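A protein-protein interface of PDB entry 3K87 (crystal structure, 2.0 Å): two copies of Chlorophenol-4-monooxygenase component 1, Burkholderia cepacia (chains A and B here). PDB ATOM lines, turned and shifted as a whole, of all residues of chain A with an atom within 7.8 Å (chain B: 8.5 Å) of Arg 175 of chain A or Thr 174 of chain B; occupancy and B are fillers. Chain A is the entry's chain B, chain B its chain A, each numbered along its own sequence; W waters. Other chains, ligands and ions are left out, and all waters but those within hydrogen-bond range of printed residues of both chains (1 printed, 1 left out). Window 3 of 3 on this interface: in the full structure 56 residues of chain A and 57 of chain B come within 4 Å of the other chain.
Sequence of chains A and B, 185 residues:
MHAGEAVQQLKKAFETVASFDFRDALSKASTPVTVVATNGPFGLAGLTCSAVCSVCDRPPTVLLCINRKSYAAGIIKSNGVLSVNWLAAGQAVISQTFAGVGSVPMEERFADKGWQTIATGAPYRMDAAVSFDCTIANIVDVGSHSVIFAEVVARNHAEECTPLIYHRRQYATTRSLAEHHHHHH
The backbone carbonyl oxygen (O) of Thr 173 of chain B is in hydrogen-bond range of the backbone NH (N) of Arg 175 of chain A (2.8 Å). O of Thr 174 of chain B sits at hydrogen-bond distance from NH1 of Arg 175 of chain A (2.9 Å). The backbone carbonyl oxygen (O) of Thr 173 of chain A sits at hydrogen-bond distance from the backbone NH (N) of Arg 175 of chain B, at 2.9 Å. The guanidinium group (NE) of Arg 175 of chain B lies within hydrogen-bond range of the backbone carbonyl oxygen (O) of Thr 174 of chain A (3.3 Å).
OG1 of Thr 173 of chain B sits at hydrogen-bond distance from OG1 of Thr 162 of chain B (2.9 Å). The side-chain hydroxyl (OG1) of Thr 173 of chain B is in hydrogen-bond range of the backbone carbonyl oxygen (O) of Pro 163 of chain B, at 2.6 Å. The backbone carbonyl oxygen (O) of Ile 165 of chain B is in hydrogen-bond range of the backbone NH (N) of Ala 172 of chain B (2.8 Å). The backbone carbonyl oxygen (O) of Pro 163 of chain A is in hydrogen-bond range of the side-chain hydroxyl (OG1) of Thr 173 of chain A (2.6 Å). O of Ala 172 of chain A sits at hydrogen-bond distance from N of Ile 165 of chain A, 2.5 Å away. O of His 167 of chain A sits at hydrogen-bond distance from NE2 of Gln 170 of chain A, 3.1 Å away.
Among the printed residues, pairs that only touch across the chains: Arg 175 of chain A with Ala 172 of chain B (3.1 Å), Thr 174 of chain A with Ala 172 of chain B (3.2 Å), Ser 30 of chain A with Pro 163 of chain B (3.3 Å), Thr 174 of chain A with Thr 173 of chain B (3.3 Å), Ser 30 of chain A with Ile 165 of chain B (3.3 Å), Ala 172 of chain A with Arg 175 of chain B (3.3 Å), Thr 173 of chain A with Thr 174 of chain B (3.3 Å), Pro 163 of chain A with Ser 30 of chain B (3.3 Å), Leu 177 of chain A with Ala 172 of chain B (3.3 Å), His 167 of chain A with Pro 163 of chain B (3.5 Å), Ala 172 of chain A with Leu 177 of chain B (3.5 Å), Leu 177 of chain A with Thr 173 of chain B (3.6 Å), Leu 177 of chain A with Tyr 171 of chain B (3.7 Å), Pro 163 of chain A with His 167 of chain B (3.7 Å), Tyr 171 of chain A with Leu 177 of chain B (3.7 Å), Thr 173 of chain A with Leu 177 of chain B (3.7 Å), Ile 165 of chain A with Thr 174 of chain B (3.9 Å), Leu 177 of chain A with Leu 164 of chain B (3.9 Å), Leu 177 of chain A with Ala 89 of chain B (3.9 Å), Arg 175 of chain A with Arg 175 of chain B (3.9 Å), Leu 164 of chain A with Leu 177 of chain B (3.99 Å), His 167 of chain A with Cys 161 of chain B (3.99 Å) and Thr 173 of chain A with Thr 173 of chain B (3.99 Å).
Of chain B, only Ala 172, Thr 173, Thr 174 and Arg 175 come within 4 Å of Arg 175 of chain A. Thr 174 of chain B touches just these residues of chain A: Ile 165, Thr 173 and Arg 175. Of the printed residues of chain A, Cys 161 of chain B touches His 167 (3.99 Å). Of the printed residues of chain B, His 167 of chain A touches Cys 161 (3.99 Å) and Pro 163 (3.5 Å). Printed residues of chain A within 4 Å of Tyr 171 of chain B: Leu 177. Printed residues of chain A within 4 Å of Thr 173 of chain B: Thr 173, Thr 174, Arg 175 and Leu 177. Printed residues of chain A within 4 Å of Ala 89 of chain B: Leu 177 (3.9 Å). Gln 170 of chain B touches none of the printed residues of chain A. Ser 176 of chain B touches none of the printed residues of chain A. The nearest residue of chain B that does not touch Arg 175 of chain A is Tyr 171 of chain B (5.0 Å). The nearest residue of chain A that does not touch Thr 174 of chain B is Ala 172 of chain A (4.1 Å). The nearest printed residue of chain A that does not touch Ala 172 of chain B is Ser 176 of chain A (4.8 Å).
Printed residues of chain B that touch a printed residue of chain A: Ser 30, Ala 89, Cys 161, Pro 163, Leu 164, Ile 165, His 167, Tyr 171, Ala 172, Thr 173, Thr 174, Arg 175 and Leu 177. Of the 16 printed residues of chain A, 11 touch a printed residue of chain B. Printed residues of chain A that touch a printed residue of chain B: Ser 30, Pro 163, Leu 164, Ile 165, His 167, Tyr 171, Ala 172, Thr 173, Thr 174, Arg 175 and Leu 177. Hydrophobic or aromatic side chains of chain A within 4 Å of the printed part of chain B: Pro 163, Leu 164, Ile 165, His 167, Tyr 171, Ala 172 and Leu 177. Among the printed residues, 27 pairs touch across the chains. Among the printed residues, no Asp or Glu carboxylate lies within 4 Å of a Lys or Arg side-chain nitrogen of the other chain.
Tyr 171 of chain A touches Leu 177 of chain B, and with the chains exchanged Leu 177 of chain A touches Tyr 171 of chain B. Ala 172 of chain A touches Leu 177 of chain B, and with the chains exchanged Leu 177 of chain A touches Ala 172 of chain B. Thr 173 of chain A touches Thr 174 of chain B, and with the chains exchanged Thr 174 of chain A touches Thr 173 of chain B. Arg 175 of chain B touches its own counterpart, Arg 175 of chain A. Of the 27 pairs that touch across the chains among the printed residues, 22 have their exchanged pair printed and touching as well.
Water W1 bridges N of Leu 177 of chain B (2.4 Å) and O of Tyr 171 of chain A (2.6 Å).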
ATOM      1  N   SER A  30      -8.200 -18.525  27.471  1.00  0.00           N
ATOM      2  CA  SER A  30      -8.376 -17.207  28.084  1.00  0.00           C
ATOM      3  C   SER A  30      -9.720 -17.172  28.813  1.00  0.00           C
ATOM      4  O   SER A  30     -10.631 -17.986  28.527  1.00  0.00           O
ATOM      5  CB  SER A  30      -8.331 -16.097  27.054  1.00  0.00           C
ATOM      6  OG  SER A  30      -9.429 -16.215  26.154  1.00  0.00           O
ATOM      7  N   THR A  31      -9.825 -16.266  29.784  1.00  0.00           N
ATOM      8  CA  THR A  31     -11.046 -16.112  30.564  1.00  0.00           C
ATOM      9  C   THR A  31     -11.218 -14.631  30.902  1.00  0.00           C
ATOM     10  O   THR A  31     -10.217 -13.893  30.990  1.00  0.00           O
ATOM     11  CB  THR A  31     -10.887 -16.803  31.935  1.00  0.00           C
ATOM     12  OG1 THR A  31      -9.780 -16.211  32.628  1.00  0.00           O
ATOM     13  CG2 THR A  31     -10.641 -18.331  31.795  1.00  0.00           C
ATOM     14  N   THR A 162     -14.790  -2.295  28.997  1.00  0.00           N
ATOM     15  CA  THR A 162     -13.570  -2.934  28.447  1.00  0.00           C
ATOM     16  C   THR A 162     -12.999  -3.938  29.420  1.00  0.00           C
ATOM     17  O   THR A 162     -12.684  -3.564  30.561  1.00  0.00           O
ATOM     18  CB  THR A 162     -12.451  -1.948  28.120  1.00  0.00           C
ATOM     19  OG1 THR A 162     -13.021  -0.755  27.587  1.00  0.00           O
ATOM     20  CG2 THR A 162     -11.498  -2.558  27.122  1.00  0.00           C
ATOM     21  N   PRO A 163     -12.850  -5.204  28.966  1.00  0.00           N
ATOM     22  CA  PRO A 163     -12.698  -6.333  29.882  1.00  0.00           C
ATOM     23  C   PRO A 163     -11.320  -6.462  30.449  1.00  0.00           C
ATOM     24  O   PRO A 163     -10.349  -6.261  29.734  1.00  0.00           O
ATOM     25  CB  PRO A 163     -12.959  -7.557  28.991  1.00  0.00           C
ATOM     26  CG  PRO A 163     -13.469  -7.046  27.727  1.00  0.00           C
ATOM     27  CD  PRO A 163     -13.021  -5.655  27.578  1.00  0.00           C
ATOM     28  N   LEU A 164     -11.236  -6.796  31.727  1.00  0.00           N
ATOM     29  CA  LEU A 164     -10.023  -7.428  32.220  1.00  0.00           C
ATOM     30  C   LEU A 164      -9.965  -8.904  31.744  1.00  0.00           C
ATOM     31  O   LEU A 164     -10.897  -9.714  31.977  1.00  0.00           O
ATOM     32  CB  LEU A 164      -9.982  -7.364  33.744  1.00  0.00           C
ATOM     33  CG  LEU A 164      -8.629  -7.782  34.327  1.00  0.00           C
ATOM     34  CD1 LEU A 164      -7.430  -6.970  33.738  1.00  0.00           C
ATOM     35  CD2 LEU A 164      -8.653  -7.787  35.867  1.00  0.00           C
ATOM     36  N   ILE A 165      -8.888  -9.272  31.076  1.00  0.00           N
ATOM     37  CA  ILE A 165      -8.758 -10.653  30.642  1.00  0.00           C
ATOM     38  C   ILE A 165      -7.542 -11.338  31.225  1.00  0.00           C
ATOM     39  O   ILE A 165      -6.556 -10.677  31.590  1.00  0.00           O
ATOM     40  CB  ILE A 165      -8.816 -10.721  29.111  1.00  0.00           C
ATOM     41  CG1 ILE A 165     -10.263 -10.468  28.705  1.00  0.00           C
ATOM     42  CG2 ILE A 165      -8.287 -12.101  28.593  1.00  0.00           C
ATOM     43  CD1 ILE A 165     -10.438  -9.989  27.333  1.00  0.00           C
ATOM     44  N   TYR A 166      -7.625 -12.656  31.417  1.00  0.00           N
ATOM     45  CA  TYR A 166      -6.471 -13.416  31.933  1.00  0.00           C
ATOM     46  C   TYR A 166      -6.028 -14.471  30.916  1.00  0.00           C
ATOM     47  O   TYR A 166      -6.858 -15.151  30.319  1.00  0.00           O
ATOM     48  CB  TYR A 166      -6.808 -14.124  33.241  1.00  0.00           C
ATOM     49  CG  TYR A 166      -5.606 -14.408  34.098  1.00  0.00           C
ATOM     50  CD1 TYR A 166      -4.910 -13.365  34.718  1.00  0.00           C
ATOM     51  CD2 TYR A 166      -5.173 -15.724  34.336  1.00  0.00           C
ATOM     52  CE1 TYR A 166      -3.807 -13.612  35.540  1.00  0.00           C
ATOM     53  CE2 TYR A 166      -4.057 -15.979  35.168  1.00  0.00           C
ATOM     54  CZ  TYR A 166      -3.393 -14.925  35.765  1.00  0.00           C
ATOM     55  OH  TYR A 166      -2.302 -15.155  36.557  1.00  0.00           O
ATOM     56  N   HIS A 167      -4.728 -14.615  30.705  1.00  0.00           N
ATOM     57  CA  HIS A 167      -4.276 -15.469  29.614  1.00  0.00           C
ATOM     58  C   HIS A 167      -2.811 -15.686  29.797  1.00  0.00           C
ATOM     59  O   HIS A 167      -2.090 -14.724  30.056  1.00  0.00           O
ATOM     60  CB  HIS A 167      -4.506 -14.780  28.266  1.00  0.00           C
ATOM     61  CG  HIS A 167      -4.032 -15.582  27.087  1.00  0.00           C
ATOM     62  ND1 HIS A 167      -3.347 -15.030  26.029  1.00  0.00           N
ATOM     63  CD2 HIS A 167      -4.140 -16.905  26.815  1.00  0.00           C
ATOM     64  CE1 HIS A 167      -3.057 -15.973  25.147  1.00  0.00           C
ATOM     65  NE2 HIS A 167      -3.524 -17.118  25.603  1.00  0.00           N
ATOM     66  N   GLN A 170      -1.069 -13.905  32.525  1.00  0.00           N
ATOM     67  CA  GLN A 170      -1.036 -12.473  32.690  1.00  0.00           C
ATOM     68  C   GLN A 170      -2.356 -11.807  32.386  1.00  0.00           C
ATOM     69  O   GLN A 170      -3.266 -12.378  31.733  1.00  0.00           O
ATOM     70  CB  GLN A 170       0.133 -11.838  31.934  1.00  0.00           C
ATOM     71  CG  GLN A 170       0.497 -12.534  30.644  1.00  0.00           C
ATOM     72  CD  GLN A 170      -0.406 -12.121  29.474  1.00  0.00           C
ATOM     73  OE1 GLN A 170      -1.153 -11.117  29.554  1.00  0.00           O
ATOM     74  NE2 GLN A 170      -0.333 -12.884  28.371  1.00  0.00           N
ATOM     75  N   TYR A 171      -2.455 -10.595  32.900  1.00  0.00           N
ATOM     76  CA  TYR A 171      -3.588  -9.734  32.616  1.00  0.00           C
ATOM     77  C   TYR A 171      -3.503  -9.150  31.221  1.00  0.00           C
ATOM     78  O   TYR A 171      -2.427  -8.892  30.681  1.00  0.00           O
ATOM     79  CB  TYR A 171      -3.689  -8.631  33.671  1.00  0.00           C
ATOM     80  CG  TYR A 171      -4.002  -9.185  35.054  1.00  0.00           C
ATOM     81  CD1 TYR A 171      -5.249  -9.761  35.325  1.00  0.00           C
ATOM     82  CD2 TYR A 171      -3.064  -9.135  36.082  1.00  0.00           C
ATOM     83  CE1 TYR A 171      -5.560 -10.254  36.589  1.00  0.00           C
ATOM     84  CE2 TYR A 171      -3.363  -9.639  37.363  1.00  0.00           C
ATOM     85  CZ  TYR A 171      -4.627 -10.193  37.595  1.00  0.00           C
ATOM     86  OH  TYR A 171      -4.965 -10.703  38.837  1.00  0.00           O
ATOM     87  N   ALA A 172      -4.665  -8.945  30.650  1.00  0.00           N
ATOM     88  CA  ALA A 172      -4.789  -8.337  29.343  1.00  0.00           C
ATOM     89  C   ALA A 172      -6.160  -7.696  29.264  1.00  0.00           C
ATOM     90  O   ALA A 172      -7.009  -7.833  30.176  1.00  0.00           O
ATOM     91  CB  ALA A 172      -4.643  -9.387  28.230  1.00  0.00           C
ATOM     92  N   THR A 173      -6.373  -7.014  28.150  1.00  0.00           N
ATOM     93  CA  THR A 173      -7.675  -6.525  27.814  1.00  0.00           C
ATOM     94  C   THR A 173      -7.833  -6.758  26.341  1.00  0.00           C
ATOM     95  O   THR A 173      -7.011  -7.433  25.729  1.00  0.00           O
ATOM     96  CB  THR A 173      -7.841  -5.062  28.130  1.00  0.00           C
ATOM     97  OG1 THR A 173      -9.216  -4.722  27.915  1.00  0.00           O
ATOM     98  CG2 THR A 173      -6.897  -4.183  27.237  1.00  0.00           C
ATOM     99  N   THR A 174      -8.903  -6.213  25.783  1.00  0.00           N
ATOM    100  CA  THR A 174      -9.316  -6.565  24.434  1.00  0.00           C
ATOM    101  C   THR A 174      -8.781  -5.587  23.377  1.00  0.00           C
ATOM    102  O   THR A 174      -8.500  -4.416  23.677  1.00  0.00           O
ATOM    103  CB  THR A 174     -10.838  -6.553  24.352  1.00  0.00           C
ATOM    104  OG1 THR A 174     -11.243  -6.652  22.989  1.00  0.00           O
ATOM    105  CG2 THR A 174     -11.354  -5.273  24.864  1.00  0.00           C
ATOM    106  N   ARG A 175      -8.685  -6.090  22.146  1.00  0.00           N
ATOM    107  CA  ARG A 175      -8.326  -5.321  20.965  1.00  0.00           C
ATOM    108  C   ARG A 175      -9.213  -5.798  19.809  1.00  0.00           C
ATOM    109  O   ARG A 175      -9.675  -6.947  19.796  1.00  0.00           O
ATOM    110  CB  ARG A 175      -6.865  -5.604  20.610  1.00  0.00           C
ATOM    111  CG  ARG A 175      -6.359  -4.919  19.355  1.00  0.00           C
ATOM    112  CD  ARG A 175      -5.629  -5.885  18.432  1.00  0.00           C
ATOM    113  NE  ARG A 175      -4.826  -6.861  19.160  1.00  0.00           N
ATOM    114  CZ  ARG A 175      -3.505  -6.985  19.051  1.00  0.00           C
ATOM    115  NH1 ARG A 175      -2.855  -7.924  19.750  1.00  0.00           N
ATOM    116  NH2 ARG A 175      -2.835  -6.174  18.233  1.00  0.00           N
ATOM    117  N   SER A 176      -9.436  -4.937  18.822  1.00  0.00           N
ATOM    118  CA  SER A 176     -10.144  -5.354  17.609  1.00  0.00           C
ATOM    119  C   SER A 176      -9.308  -6.332  16.756  1.00  0.00           C
ATOM    120  O   SER A 176      -8.071  -6.396  16.864  1.00  0.00           O
ATOM    121  CB  SER A 176     -10.556  -4.125  16.794  1.00  0.00           C
ATOM    122  OG  SER A 176     -10.911  -4.486  15.471  1.00  0.00           O
ATOM    123  N   LEU A 177      -9.985  -7.119  15.924  1.00  0.00           N
ATOM    124  CA  LEU A 177      -9.276  -8.053  15.064  1.00  0.00           C
ATOM    125  C   LEU A 177      -8.938  -7.336  13.770  1.00  0.00           C
ATOM    126  O   LEU A 177      -9.667  -6.429  13.375  1.00  0.00           O
ATOM    127  CB  LEU A 177     -10.132  -9.276  14.765  1.00  0.00           C
ATOM    128  CG  LEU A 177     -10.639 -10.160  15.905  1.00  0.00           C
ATOM    129  CD1 LEU A 177     -11.460 -11.295  15.283  1.00  0.00           C
ATOM    130  CD2 LEU A 177      -9.498 -10.736  16.694  1.00  0.00           C
ATOM    131  N   SER B  30     -17.194 -10.452  28.866  1.00  0.00           N
ATOM    132  CA  SER B  30     -16.493 -11.020  27.733  1.00  0.00           C
ATOM    133  C   SER B  30     -16.345 -12.518  27.993  1.00  0.00           C
ATOM    134  O   SER B  30     -16.502 -12.957  29.131  1.00  0.00           O
ATOM    135  CB  SER B  30     -15.143 -10.332  27.524  1.00  0.00           C
ATOM    136  OG  SER B  30     -14.274 -10.575  28.624  1.00  0.00           O
ATOM    137  N   ALA B  89      -7.235 -16.130  17.715  1.00  0.00           N
ATOM    138  CA  ALA B  89      -7.656 -14.874  17.072  1.00  0.00           C
ATOM    139  C   ALA B  89      -8.018 -14.989  15.569  1.00  0.00           C
ATOM    140  O   ALA B  89      -8.922 -14.301  15.102  1.00  0.00           O
ATOM    141  CB  ALA B  89      -6.620 -13.770  17.305  1.00  0.00           C
ATOM    142  N   CYS B 161      -1.083 -18.726  19.437  1.00  0.00           N
ATOM    143  CA  CYS B 161      -2.471 -18.305  19.415  1.00  0.00           C
ATOM    144  C   CYS B 161      -2.923 -17.386  20.553  1.00  0.00           C
ATOM    145  O   CYS B 161      -3.320 -17.856  21.640  1.00  0.00           O
ATOM    146  CB  CYS B 161      -3.360 -19.551  19.340  1.00  0.00           C
ATOM    147  SG  CYS B 161      -2.485 -20.882  18.538  1.00  0.00           S
ATOM    148  N   THR B 162      -2.904 -16.082  20.291  1.00  0.00           N
ATOM    149  CA  THR B 162      -3.730 -15.198  21.096  1.00  0.00           C
ATOM    150  C   THR B 162      -5.191 -15.623  20.833  1.00  0.00           C
ATOM    151  O   THR B 162      -5.479 -16.248  19.790  1.00  0.00           O
ATOM    152  CB  THR B 162      -3.477 -13.707  20.788  1.00  0.00           C
ATOM    153  OG1 THR B 162      -4.046 -13.365  19.514  1.00  0.00           O
ATOM    154  CG2 THR B 162      -1.975 -13.403  20.799  1.00  0.00           C
ATOM    155  N   PRO B 163      -6.082 -15.350  21.804  1.00  0.00           N
ATOM    156  CA  PRO B 163      -7.434 -15.948  21.849  1.00  0.00           C
ATOM    157  C   PRO B 163      -8.435 -15.223  20.972  1.00  0.00           C
ATOM    158  O   PRO B 163      -8.280 -14.031  20.681  1.00  0.00           O
ATOM    159  CB  PRO B 163      -7.890 -15.744  23.305  1.00  0.00           C
ATOM    160  CG  PRO B 163      -6.876 -14.769  23.950  1.00  0.00           C
ATOM    161  CD  PRO B 163      -5.627 -14.809  23.105  1.00  0.00           C
ATOM    162  N   LEU B 164      -9.481 -15.933  20.567  1.00  0.00           N
ATOM    163  CA  LEU B 164     -10.624 -15.251  19.996  1.00  0.00           C
ATOM    164  C   LEU B 164     -11.491 -14.940  21.195  1.00  0.00           C
ATOM    165  O   LEU B 164     -11.777 -15.830  22.017  1.00  0.00           O
ATOM    166  CB  LEU B 164     -11.378 -16.158  19.046  1.00  0.00           C
ATOM    167  CG  LEU B 164     -12.608 -15.576  18.387  1.00  0.00           C
ATOM    168  CD1 LEU B 164     -12.179 -14.458  17.453  1.00  0.00           C
ATOM    169  CD2 LEU B 164     -13.277 -16.702  17.580  1.00  0.00           C
ATOM    170  N   ILE B 165     -11.908 -13.697  21.309  1.00  0.00           N
ATOM    171  CA  ILE B 165     -12.663 -13.259  22.457  1.00  0.00           C
ATOM    172  C   ILE B 165     -14.000 -12.746  21.914  1.00  0.00           C
ATOM    173  O   ILE B 165     -14.057 -12.226  20.798  1.00  0.00           O
ATOM    174  CB  ILE B 165     -11.935 -12.090  23.194  1.00  0.00           C
ATOM    175  CG1 ILE B 165     -10.536 -12.518  23.677  1.00  0.00           C
ATOM    176  CG2 ILE B 165     -12.855 -11.426  24.291  1.00  0.00           C
ATOM    177  CD1 ILE B 165     -10.551 -13.395  24.855  1.00  0.00           C
ATOM    178  N   HIS B 167     -17.213 -10.086  22.832  1.00  0.00           N
ATOM    179  CA  HIS B 167     -17.551  -8.976  23.751  1.00  0.00           C
ATOM    180  C   HIS B 167     -18.328  -7.928  23.018  1.00  0.00           C
ATOM    181  O   HIS B 167     -17.935  -7.520  21.906  1.00  0.00           O
ATOM    182  CB  HIS B 167     -16.274  -8.353  24.343  1.00  0.00           C
ATOM    183  CG  HIS B 167     -16.524  -7.185  25.253  1.00  0.00           C
ATOM    184  ND1 HIS B 167     -15.933  -5.954  25.068  1.00  0.00           N
ATOM    185  CD2 HIS B 167     -17.313  -7.067  26.350  1.00  0.00           C
ATOM    186  CE1 HIS B 167     -16.329  -5.129  26.023  1.00  0.00           C
ATOM    187  NE2 HIS B 167     -17.168  -5.777  26.810  1.00  0.00           N
ATOM    188  N   GLN B 170     -19.213  -8.600  19.442  1.00  0.00           N
ATOM    189  CA  GLN B 170     -18.205  -8.622  18.400  1.00  0.00           C
ATOM    190  C   GLN B 170     -17.047  -9.511  18.801  1.00  0.00           C
ATOM    191  O   GLN B 170     -16.785  -9.700  19.989  1.00  0.00           O
ATOM    192  CB  GLN B 170     -17.649  -7.211  18.158  1.00  0.00           C
ATOM    193  CG  GLN B 170     -18.620  -6.211  17.518  1.00  0.00           C
ATOM    194  CD  GLN B 170     -18.062  -4.805  17.603  1.00  0.00           C
ATOM    195  OE1 GLN B 170     -17.031  -4.496  16.989  1.00  0.00           O
ATOM    196  NE2 GLN B 170     -18.715  -3.950  18.392  1.00  0.00           N
ATOM    197  N   TYR B 171     -16.341 -10.036  17.803  1.00  0.00           N
ATOM    198  CA  TYR B 171     -15.116 -10.762  18.064  1.00  0.00           C
ATOM    199  C   TYR B 171     -13.997  -9.792  18.368  1.00  0.00           C
ATOM    200  O   TYR B 171     -14.018  -8.644  17.921  1.00  0.00           O
ATOM    201  CB  TYR B 171     -14.742 -11.651  16.889  1.00  0.00           C
ATOM    202  CG  TYR B 171     -15.776 -12.729  16.649  1.00  0.00           C
ATOM    203  CD1 TYR B 171     -15.881 -13.822  17.513  1.00  0.00           C
ATOM    204  CD2 TYR B 171     -16.673 -12.635  15.584  1.00  0.00           C
ATOM    205  CE1 TYR B 171     -16.841 -14.815  17.293  1.00  0.00           C
ATOM    206  CE2 TYR B 171     -17.645 -13.613  15.370  1.00  0.00           C
ATOM    207  CZ  TYR B 171     -17.714 -14.686  16.233  1.00  0.00           C
ATOM    208  OH  TYR B 171     -18.652 -15.626  16.042  1.00  0.00           O
ATOM    209  N   ALA B 172     -13.019 -10.272  19.127  1.00  0.00           N
ATOM    210  CA  ALA B 172     -11.866  -9.478  19.448  1.00  0.00           C
ATOM    211  C   ALA B 172     -10.699 -10.424  19.773  1.00  0.00           C
ATOM    212  O   ALA B 172     -10.811 -11.654  19.635  1.00  0.00           O
ATOM    213  CB  ALA B 172     -12.190  -8.602  20.612  1.00  0.00           C
ATOM    214  N   THR B 173      -9.582  -9.857  20.219  1.00  0.00           N
ATOM    215  CA  THR B 173      -8.490 -10.663  20.728  1.00  0.00           C
ATOM    216  C   THR B 173      -7.838  -9.880  21.839  1.00  0.00           C
ATOM    217  O   THR B 173      -8.413  -8.914  22.299  1.00  0.00           O
ATOM    218  CB  THR B 173      -7.523 -11.166  19.619  1.00  0.00           C
ATOM    219  OG1 THR B 173      -6.579 -12.085  20.189  1.00  0.00           O
ATOM    220  CG2 THR B 173      -6.775  -9.997  18.936  1.00  0.00           C
ATOM    221  N   THR B 174      -6.668 -10.296  22.298  1.00  0.00           N
ATOM    222  CA  THR B 174      -6.086  -9.653  23.460  1.00  0.00           C
ATOM    223  C   THR B 174      -4.961  -8.684  23.092  1.00  0.00           C
ATOM    224  O   THR B 174      -4.348  -8.794  22.039  1.00  0.00           O
ATOM    225  CB  THR B 174      -5.484 -10.697  24.411  1.00  0.00           C
ATOM    226  OG1 THR B 174      -4.777 -11.664  23.629  1.00  0.00           O
ATOM    227  CG2 THR B 174      -6.591 -11.396  25.206  1.00  0.00           C
ATOM    228  N   ARG B 175      -4.693  -7.759  23.998  1.00  0.00           N
ATOM    229  CA  ARG B 175      -3.512  -6.916  23.954  1.00  0.00           C
ATOM    230  C   ARG B 175      -3.082  -6.689  25.394  1.00  0.00           C
ATOM    231  O   ARG B 175      -3.906  -6.789  26.324  1.00  0.00           O
ATOM    232  CB  ARG B 175      -3.828  -5.590  23.277  1.00  0.00           C
ATOM    233  CG  ARG B 175      -4.901  -4.801  23.938  1.00  0.00           C
ATOM    234  CD  ARG B 175      -4.962  -3.391  23.346  1.00  0.00           C
ATOM    235  NE  ARG B 175      -5.828  -2.523  24.142  1.00  0.00           N
ATOM    236  CZ  ARG B 175      -5.417  -1.857  25.219  1.00  0.00           C
ATOM    237  NH1 ARG B 175      -6.273  -1.092  25.888  1.00  0.00           N
ATOM    238  NH2 ARG B 175      -4.149  -1.950  25.624  1.00  0.00           N
ATOM    239  N   SER B 176      -1.794  -6.416  25.596  1.00  0.00           N
ATOM    240  CA  SER B 176      -1.280  -6.151  26.933  1.00  0.00           C
ATOM    241  C   SER B 176      -1.927  -4.883  27.481  1.00  0.00           C
ATOM    242  O   SER B 176      -2.369  -4.010  26.706  1.00  0.00           O
ATOM    243  CB  SER B 176       0.239  -5.989  26.897  1.00  0.00           C
ATOM    244  OG  SER B 176       0.590  -4.676  26.482  1.00  0.00           O
ATOM    245  N   LEU B 177      -2.021  -4.805  28.811  1.00  0.00           N
ATOM    246  CA  LEU B 177      -2.566  -3.643  29.481  1.00  0.00           C
ATOM    247  C   LEU B 177      -1.525  -2.524  29.464  1.00  0.00           C
ATOM    248  O   LEU B 177      -1.853  -1.368  29.179  1.00  0.00           O
ATOM    249  CB  LEU B 177      -2.918  -3.973  30.923  1.00  0.00           C
ATOM    250  CG  LEU B 177      -3.970  -5.012  31.323  1.00  0.00           C
ATOM    251  CD1 LEU B 177      -4.060  -5.046  32.821  1.00  0.00           C
ATOM    252  CD2 LEU B 177      -5.299  -4.626  30.791  1.00  0.00           C
HETATM  253  O   HOH W   1      -1.148  -6.692  30.013  1.00  0.00           O
